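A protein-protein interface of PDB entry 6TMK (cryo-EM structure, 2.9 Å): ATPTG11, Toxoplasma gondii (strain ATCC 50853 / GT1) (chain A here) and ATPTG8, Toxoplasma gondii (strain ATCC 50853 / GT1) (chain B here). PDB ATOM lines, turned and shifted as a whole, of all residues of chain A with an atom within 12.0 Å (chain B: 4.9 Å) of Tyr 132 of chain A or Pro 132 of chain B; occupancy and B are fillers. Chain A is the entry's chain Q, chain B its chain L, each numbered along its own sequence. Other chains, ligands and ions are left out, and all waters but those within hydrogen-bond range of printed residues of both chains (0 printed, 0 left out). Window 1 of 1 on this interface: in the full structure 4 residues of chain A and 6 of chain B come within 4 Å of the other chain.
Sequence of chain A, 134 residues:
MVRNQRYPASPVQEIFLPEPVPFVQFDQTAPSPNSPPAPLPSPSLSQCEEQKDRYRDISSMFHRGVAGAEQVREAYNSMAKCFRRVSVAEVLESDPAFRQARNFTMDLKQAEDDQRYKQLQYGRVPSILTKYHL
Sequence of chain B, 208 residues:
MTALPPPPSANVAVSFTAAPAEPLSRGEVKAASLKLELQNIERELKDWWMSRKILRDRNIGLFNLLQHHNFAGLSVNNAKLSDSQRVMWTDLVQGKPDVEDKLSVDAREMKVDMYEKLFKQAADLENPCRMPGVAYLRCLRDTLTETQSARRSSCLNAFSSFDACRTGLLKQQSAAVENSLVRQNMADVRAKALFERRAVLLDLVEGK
The backbone carbonyl oxygen (O) of Pro 128 of chain B lies within hydrogen-bond range of the side-chain hydroxyl (OH) of Tyr 132 of chain A (3.2 Å). The backbone carbonyl oxygen (O) of Tyr 132 of chain A sits at hydrogen-bond distance from the side-chain hydroxyl (OG) of Ser 161 of chain B (2.7 Å).
O of Leu 129 of chain A lies within hydrogen-bond range of N of Leu 134 of chain A.
CG2 of Ile 128 of chain A touches SD of Met 131 of chain B (3.5 Å). Tyr 132 of chain A touches Met 131 of chain B. Tyr 132 of chain A touches Pro 132 of chain B. Leu 134 of chain A touches Ala 158 of chain B. CD2 of Leu 134 of chain A touches OG of Ser 161 of chain B (3.6 Å).
Of chain A, only Tyr 132 comes within 4 Å of Pro 132 of chain B. Pro 128 of chain B touches just one residue of chain A: Tyr 132 (3.2 Å). No residue of chain A comes within 4 Å of Cys 129 of chain B. Met 131 of chain B touches two residues of chain A. No residue of chain A comes within 4 Å of Val 134 of chain B. Printed residues of chain B within 4 Å of Leu 134 of chain A: Ala 158 and Ser 161. Printed residues of chain B within 4 Å of Ile 128 of chain A: Met 131. Leu 129 of chain A touches none of the printed residues of chain B. Tyr 136 of chain B touches none of the printed residues of chain A. The nearest printed residue of chain B that does not touch Tyr 132 of chain A is Cys 129 of chain B (5.4 Å). The nearest residue of chain A that does not touch Pro 132 of chain B is Leu 134 of chain A (4.7 Å).
Of the 9 printed residues of chain A, 3 touch a printed residue of chain B. Printed residues of chain A that touch a printed residue of chain B: Ile 128, Tyr 132 and Leu 134. Hydrophobic or aromatic side chains of chain A that line the printed part of chain B: Ile 128, Tyr 132 and Leu 134. Among the printed residues, 7 pairs touch across the chains. Among the printed residues, no Asp or Glu carboxylate lies within 4 Å of a Lys or Arg side-chain nitrogen of the other chain.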
ATOM      1  N   PRO A 126     -16.456  15.784   4.090  1.00  0.00           N
ATOM      2  CA  PRO A 126     -17.672  15.042   3.739  1.00  0.00           C
ATOM      3  C   PRO A 126     -18.830  15.321   4.680  1.00  0.00           C
ATOM      4  O   PRO A 126     -18.679  16.032   5.676  1.00  0.00           O
ATOM      5  CB  PRO A 126     -17.228  13.578   3.825  1.00  0.00           C
ATOM      6  CG  PRO A 126     -15.766  13.613   3.689  1.00  0.00           C
ATOM      7  CD  PRO A 126     -15.323  14.878   4.329  1.00  0.00           C
ATOM      8  N   SER A 127     -19.990  14.761   4.366  1.00  0.00           N
ATOM      9  CA  SER A 127     -21.174  14.976   5.177  1.00  0.00           C
ATOM     10  C   SER A 127     -21.160  14.069   6.398  1.00  0.00           C
ATOM     11  O   SER A 127     -20.618  12.961   6.375  1.00  0.00           O
ATOM     12  CB  SER A 127     -22.440  14.726   4.363  1.00  0.00           C
ATOM     13  OG  SER A 127     -23.564  14.589   5.209  1.00  0.00           O
ATOM     14  N   ILE A 128     -21.764  14.562   7.479  1.00  0.00           N
ATOM     15  CA  ILE A 128     -21.792  13.829   8.735  1.00  0.00           C
ATOM     16  C   ILE A 128     -22.699  12.611   8.694  1.00  0.00           C
ATOM     17  O   ILE A 128     -22.666  11.796   9.620  1.00  0.00           O
ATOM     18  CB  ILE A 128     -22.215  14.791   9.861  1.00  0.00           C
ATOM     19  CG1 ILE A 128     -22.021  14.140  11.226  1.00  0.00           C
ATOM     20  CG2 ILE A 128     -23.646  15.236   9.672  1.00  0.00           C
ATOM     21  CD1 ILE A 128     -21.894  15.140  12.335  1.00  0.00           C
ATOM     22  N   LEU A 129     -23.512  12.468   7.649  1.00  0.00           N
ATOM     23  CA  LEU A 129     -24.391  11.314   7.525  1.00  0.00           C
ATOM     24  C   LEU A 129     -23.657  10.063   7.068  1.00  0.00           C
ATOM     25  O   LEU A 129     -24.167   8.952   7.253  1.00  0.00           O
ATOM     26  CB  LEU A 129     -25.516  11.630   6.545  1.00  0.00           C
ATOM     27  CG  LEU A 129     -26.386  12.823   6.921  1.00  0.00           C
ATOM     28  CD1 LEU A 129     -27.045  13.401   5.698  1.00  0.00           C
ATOM     29  CD2 LEU A 129     -27.434  12.407   7.925  1.00  0.00           C
ATOM     30  N   THR A 130     -22.471  10.216   6.482  1.00  0.00           N
ATOM     31  CA  THR A 130     -21.659   9.059   6.142  1.00  0.00           C
ATOM     32  C   THR A 130     -21.237   8.282   7.376  1.00  0.00           C
ATOM     33  O   THR A 130     -20.891   7.102   7.266  1.00  0.00           O
ATOM     34  CB  THR A 130     -20.427   9.509   5.365  1.00  0.00           C
ATOM     35  OG1 THR A 130     -19.657  10.409   6.167  1.00  0.00           O
ATOM     36  CG2 THR A 130     -20.847  10.222   4.102  1.00  0.00           C
ATOM     37  N   LYS A 131     -21.258   8.920   8.545  1.00  0.00           N
ATOM     38  CA  LYS A 131     -20.977   8.210   9.783  1.00  0.00           C
ATOM     39  C   LYS A 131     -22.039   7.158  10.062  1.00  0.00           C
ATOM     40  O   LYS A 131     -21.726   6.050  10.511  1.00  0.00           O
ATOM     41  CB  LYS A 131     -20.882   9.211  10.927  1.00  0.00           C
ATOM     42  CG  LYS A 131     -19.793  10.255  10.727  1.00  0.00           C
ATOM     43  CD  LYS A 131     -18.389   9.700  10.913  1.00  0.00           C
ATOM     44  CE  LYS A 131     -17.745   9.365   9.578  1.00  0.00           C
ATOM     45  NZ  LYS A 131     -16.329   8.949   9.714  1.00  0.00           N
ATOM     46  N   TYR A 132     -23.301   7.490   9.809  1.00  0.00           N
ATOM     47  CA  TYR A 132     -24.400   6.546   9.922  1.00  0.00           C
ATOM     48  C   TYR A 132     -24.657   5.792   8.628  1.00  0.00           C
ATOM     49  O   TYR A 132     -25.573   4.967   8.578  1.00  0.00           O
ATOM     50  CB  TYR A 132     -25.671   7.277  10.342  1.00  0.00           C
ATOM     51  CG  TYR A 132     -25.505   8.183  11.534  1.00  0.00           C
ATOM     52  CD1 TYR A 132     -25.727   7.718  12.816  1.00  0.00           C
ATOM     53  CD2 TYR A 132     -25.129   9.500  11.377  1.00  0.00           C
ATOM     54  CE1 TYR A 132     -25.582   8.540  13.902  1.00  0.00           C
ATOM     55  CE2 TYR A 132     -24.978  10.328  12.458  1.00  0.00           C
ATOM     56  CZ  TYR A 132     -25.202   9.843  13.719  1.00  0.00           C
ATOM     57  OH  TYR A 132     -25.056  10.660  14.807  1.00  0.00           O
ATOM     58  N   HIS A 133     -23.869   6.052   7.587  1.00  0.00           N
ATOM     59  CA  HIS A 133     -23.957   5.320   6.326  1.00  0.00           C
ATOM     60  C   HIS A 133     -25.311   5.536   5.650  1.00  0.00           C
ATOM     61  O   HIS A 133     -26.101   4.610   5.458  1.00  0.00           O
ATOM     62  CB  HIS A 133     -23.686   3.835   6.561  1.00  0.00           C
ATOM     63  CG  HIS A 133     -22.413   3.574   7.299  1.00  0.00           C
ATOM     64  ND1 HIS A 133     -21.178   3.930   6.802  1.00  0.00           N
ATOM     65  CD2 HIS A 133     -22.183   3.003   8.505  1.00  0.00           C
ATOM     66  CE1 HIS A 133     -20.242   3.585   7.665  1.00  0.00           C
ATOM     67  NE2 HIS A 133     -20.824   3.021   8.708  1.00  0.00           N
ATOM     68  N   LEU A 134     -25.566   6.790   5.291  1.00  0.00           N
ATOM     69  CA  LEU A 134     -26.817   7.167   4.650  1.00  0.00           C
ATOM     70  C   LEU A 134     -26.533   7.875   3.331  1.00  0.00           C
ATOM     71  O   LEU A 134     -25.811   8.872   3.296  1.00  0.00           O
ATOM     72  CB  LEU A 134     -27.651   8.068   5.563  1.00  0.00           C
ATOM     73  CG  LEU A 134     -27.699   7.660   7.031  1.00  0.00           C
ATOM     74  CD1 LEU A 134     -28.288   8.773   7.865  1.00  0.00           C
ATOM     75  CD2 LEU A 134     -28.498   6.395   7.181  1.00  0.00           C
ATOM     76  N   PRO B 128     -27.426  11.148  19.754  1.00  0.00           N
ATOM     77  CA  PRO B 128     -26.909  10.502  18.539  1.00  0.00           C
ATOM     78  C   PRO B 128     -27.989  10.002  17.594  1.00  0.00           C
ATOM     79  O   PRO B 128     -27.760   9.986  16.379  1.00  0.00           O
ATOM     80  CB  PRO B 128     -26.070   9.340  19.091  1.00  0.00           C
ATOM     81  CG  PRO B 128     -25.846   9.657  20.512  1.00  0.00           C
ATOM     82  CD  PRO B 128     -27.027  10.413  20.961  1.00  0.00           C
ATOM     83  N   CYS B 129     -29.145   9.579  18.100  1.00  0.00           N
ATOM     84  CA  CYS B 129     -30.169   8.994  17.243  1.00  0.00           C
ATOM     85  C   CYS B 129     -30.983  10.038  16.487  1.00  0.00           C
ATOM     86  O   CYS B 129     -31.802   9.667  15.632  1.00  0.00           O
ATOM     87  CB  CYS B 129     -31.106   8.121  18.079  1.00  0.00           C
ATOM     88  SG  CYS B 129     -30.284   6.958  19.191  1.00  0.00           S
ATOM     89  N   ARG B 130     -30.758  11.322  16.758  1.00  0.00           N
ATOM     90  CA  ARG B 130     -31.552  12.371  16.130  1.00  0.00           C
ATOM     91  C   ARG B 130     -31.376  12.387  14.620  1.00  0.00           C
ATOM     92  O   ARG B 130     -32.357  12.462  13.873  1.00  0.00           O
ATOM     93  CB  ARG B 130     -31.181  13.723  16.720  1.00  0.00           C
ATOM     94  CG  ARG B 130     -32.157  14.815  16.374  1.00  0.00           C
ATOM     95  CD  ARG B 130     -31.526  16.157  16.515  1.00  0.00           C
ATOM     96  NE  ARG B 130     -32.334  17.212  15.920  1.00  0.00           N
ATOM     97  CZ  ARG B 130     -33.378  17.780  16.504  1.00  0.00           C
ATOM     98  NH1 ARG B 130     -33.765  17.399  17.705  1.00  0.00           N
ATOM     99  NH2 ARG B 130     -34.042  18.730  15.879  1.00  0.00           N
ATOM    100  N   MET B 131     -30.134  12.357  14.149  1.00  0.00           N
ATOM    101  CA  MET B 131     -29.906  12.418  12.709  1.00  0.00           C
ATOM    102  C   MET B 131     -30.487  11.216  11.986  1.00  0.00           C
ATOM    103  O   MET B 131     -31.169  11.406  10.964  1.00  0.00           O
ATOM    104  CB  MET B 131     -28.408  12.563  12.431  1.00  0.00           C
ATOM    105  CG  MET B 131     -27.957  13.994  12.234  1.00  0.00           C
ATOM    106  SD  MET B 131     -26.257  14.140  11.666  1.00  0.00           S
ATOM    107  CE  MET B 131     -25.377  14.195  13.218  1.00  0.00           C
ATOM    108  N   PRO B 132     -30.261   9.979  12.429  1.00  0.00           N
ATOM    109  CA  PRO B 132     -30.930   8.847  11.779  1.00  0.00           C
ATOM    110  C   PRO B 132     -32.444   8.933  11.807  1.00  0.00           C
ATOM    111  O   PRO B 132     -33.092   8.631  10.796  1.00  0.00           O
ATOM    112  CB  PRO B 132     -30.419   7.650  12.586  1.00  0.00           C
ATOM    113  CG  PRO B 132     -29.132   8.066  13.096  1.00  0.00           C
ATOM    114  CD  PRO B 132     -29.202   9.532  13.341  1.00  0.00           C
ATOM    115  N   GLY B 133     -33.033   9.334  12.934  1.00  0.00           N
ATOM    116  CA  GLY B 133     -34.479   9.439  12.986  1.00  0.00           C
ATOM    117  C   GLY B 133     -35.021  10.464  12.014  1.00  0.00           C
ATOM    118  O   GLY B 133     -35.994  10.215  11.293  1.00  0.00           O
ATOM    119  N   VAL B 134     -34.394  11.638  11.979  1.00  0.00           N
ATOM    120  CA  VAL B 134     -34.840  12.691  11.081  1.00  0.00           C
ATOM    121  C   VAL B 134     -34.662  12.263   9.635  1.00  0.00           C
ATOM    122  O   VAL B 134     -35.496  12.567   8.777  1.00  0.00           O
ATOM    123  CB  VAL B 134     -34.092  13.998  11.384  1.00  0.00           C
ATOM    124  CG1 VAL B 134     -34.405  15.029  10.343  1.00  0.00           C
ATOM    125  CG2 VAL B 134     -34.453  14.505  12.752  1.00  0.00           C
ATOM    126  N   ALA B 135     -33.582  11.539   9.341  1.00  0.00           N
ATOM    127  CA  ALA B 135     -33.364  11.058   7.984  1.00  0.00           C
ATOM    128  C   ALA B 135     -34.440  10.064   7.573  1.00  0.00           C
ATOM    129  O   ALA B 135     -34.954  10.121   6.449  1.00  0.00           O
ATOM    130  CB  ALA B 135     -31.979  10.433   7.879  1.00  0.00           C
ATOM    131  N   TYR B 136     -34.798   9.147   8.470  1.00  0.00           N
ATOM    132  CA  TYR B 136     -35.823   8.164   8.150  1.00  0.00           C
ATOM    133  C   TYR B 136     -37.171   8.833   7.917  1.00  0.00           C
ATOM    134  O   TYR B 136     -37.896   8.488   6.975  1.00  0.00           O
ATOM    135  CB  TYR B 136     -35.921   7.125   9.262  1.00  0.00           C
ATOM    136  CG  TYR B 136     -37.020   6.121   9.045  1.00  0.00           C
ATOM    137  CD1 TYR B 136     -36.982   5.252   7.973  1.00  0.00           C
ATOM    138  CD2 TYR B 136     -38.090   6.034   9.913  1.00  0.00           C
ATOM    139  CE1 TYR B 136     -37.976   4.333   7.768  1.00  0.00           C
ATOM    140  CE2 TYR B 136     -39.091   5.118   9.714  1.00  0.00           C
ATOM    141  CZ  TYR B 136     -39.029   4.269   8.640  1.00  0.00           C
ATOM    142  OH  TYR B 136     -40.028   3.349   8.436  1.00  0.00           O
ATOM    143  N   ALA B 158     -31.711   3.714   6.123  1.00  0.00           N
ATOM    144  CA  ALA B 158     -31.768   4.661   7.228  1.00  0.00           C
ATOM    145  C   ALA B 158     -32.388   4.047   8.475  1.00  0.00           C
ATOM    146  O   ALA B 158     -31.950   4.335   9.599  1.00  0.00           O
ATOM    147  CB  ALA B 158     -32.558   5.899   6.809  1.00  0.00           C
ATOM    148  N   SER B 161     -29.705   2.210  10.631  1.00  0.00           N
ATOM    149  CA  SER B 161     -28.925   3.054  11.526  1.00  0.00           C
ATOM    150  C   SER B 161     -29.766   3.536  12.698  1.00  0.00           C
ATOM    151  O   SER B 161     -29.290   3.584  13.842  1.00  0.00           O
ATOM    152  CB  SER B 161     -28.373   4.243  10.750  1.00  0.00           C
ATOM    153  OG  SER B 161     -27.778   3.823   9.537  1.00  0.00           O
ATOM    154  N   PHE B 162     -31.016   3.913  12.430  1.00  0.00           N
ATOM    155  CA  PHE B 162     -31.894   4.356  13.503  1.00  0.00           C
ATOM    156  C   PHE B 162     -32.081   3.257  14.545  1.00  0.00           C
ATOM    157  O   PHE B 162     -31.912   3.488  15.749  1.00  0.00           O
ATOM    158  CB  PHE B 162     -33.229   4.798  12.918  1.00  0.00           C
ATOM    159  CG  PHE B 162     -34.214   5.267  13.939  1.00  0.00           C
ATOM    160  CD1 PHE B 162     -35.528   4.858  13.886  1.00  0.00           C
ATOM    161  CD2 PHE B 162     -33.829   6.127  14.946  1.00  0.00           C
ATOM    162  CE1 PHE B 162     -36.429   5.291  14.816  1.00  0.00           C
ATOM    163  CE2 PHE B 162     -34.729   6.558  15.877  1.00  0.00           C
ATOM    164  CZ  PHE B 162     -36.030   6.139  15.814  1.00  0.00           C
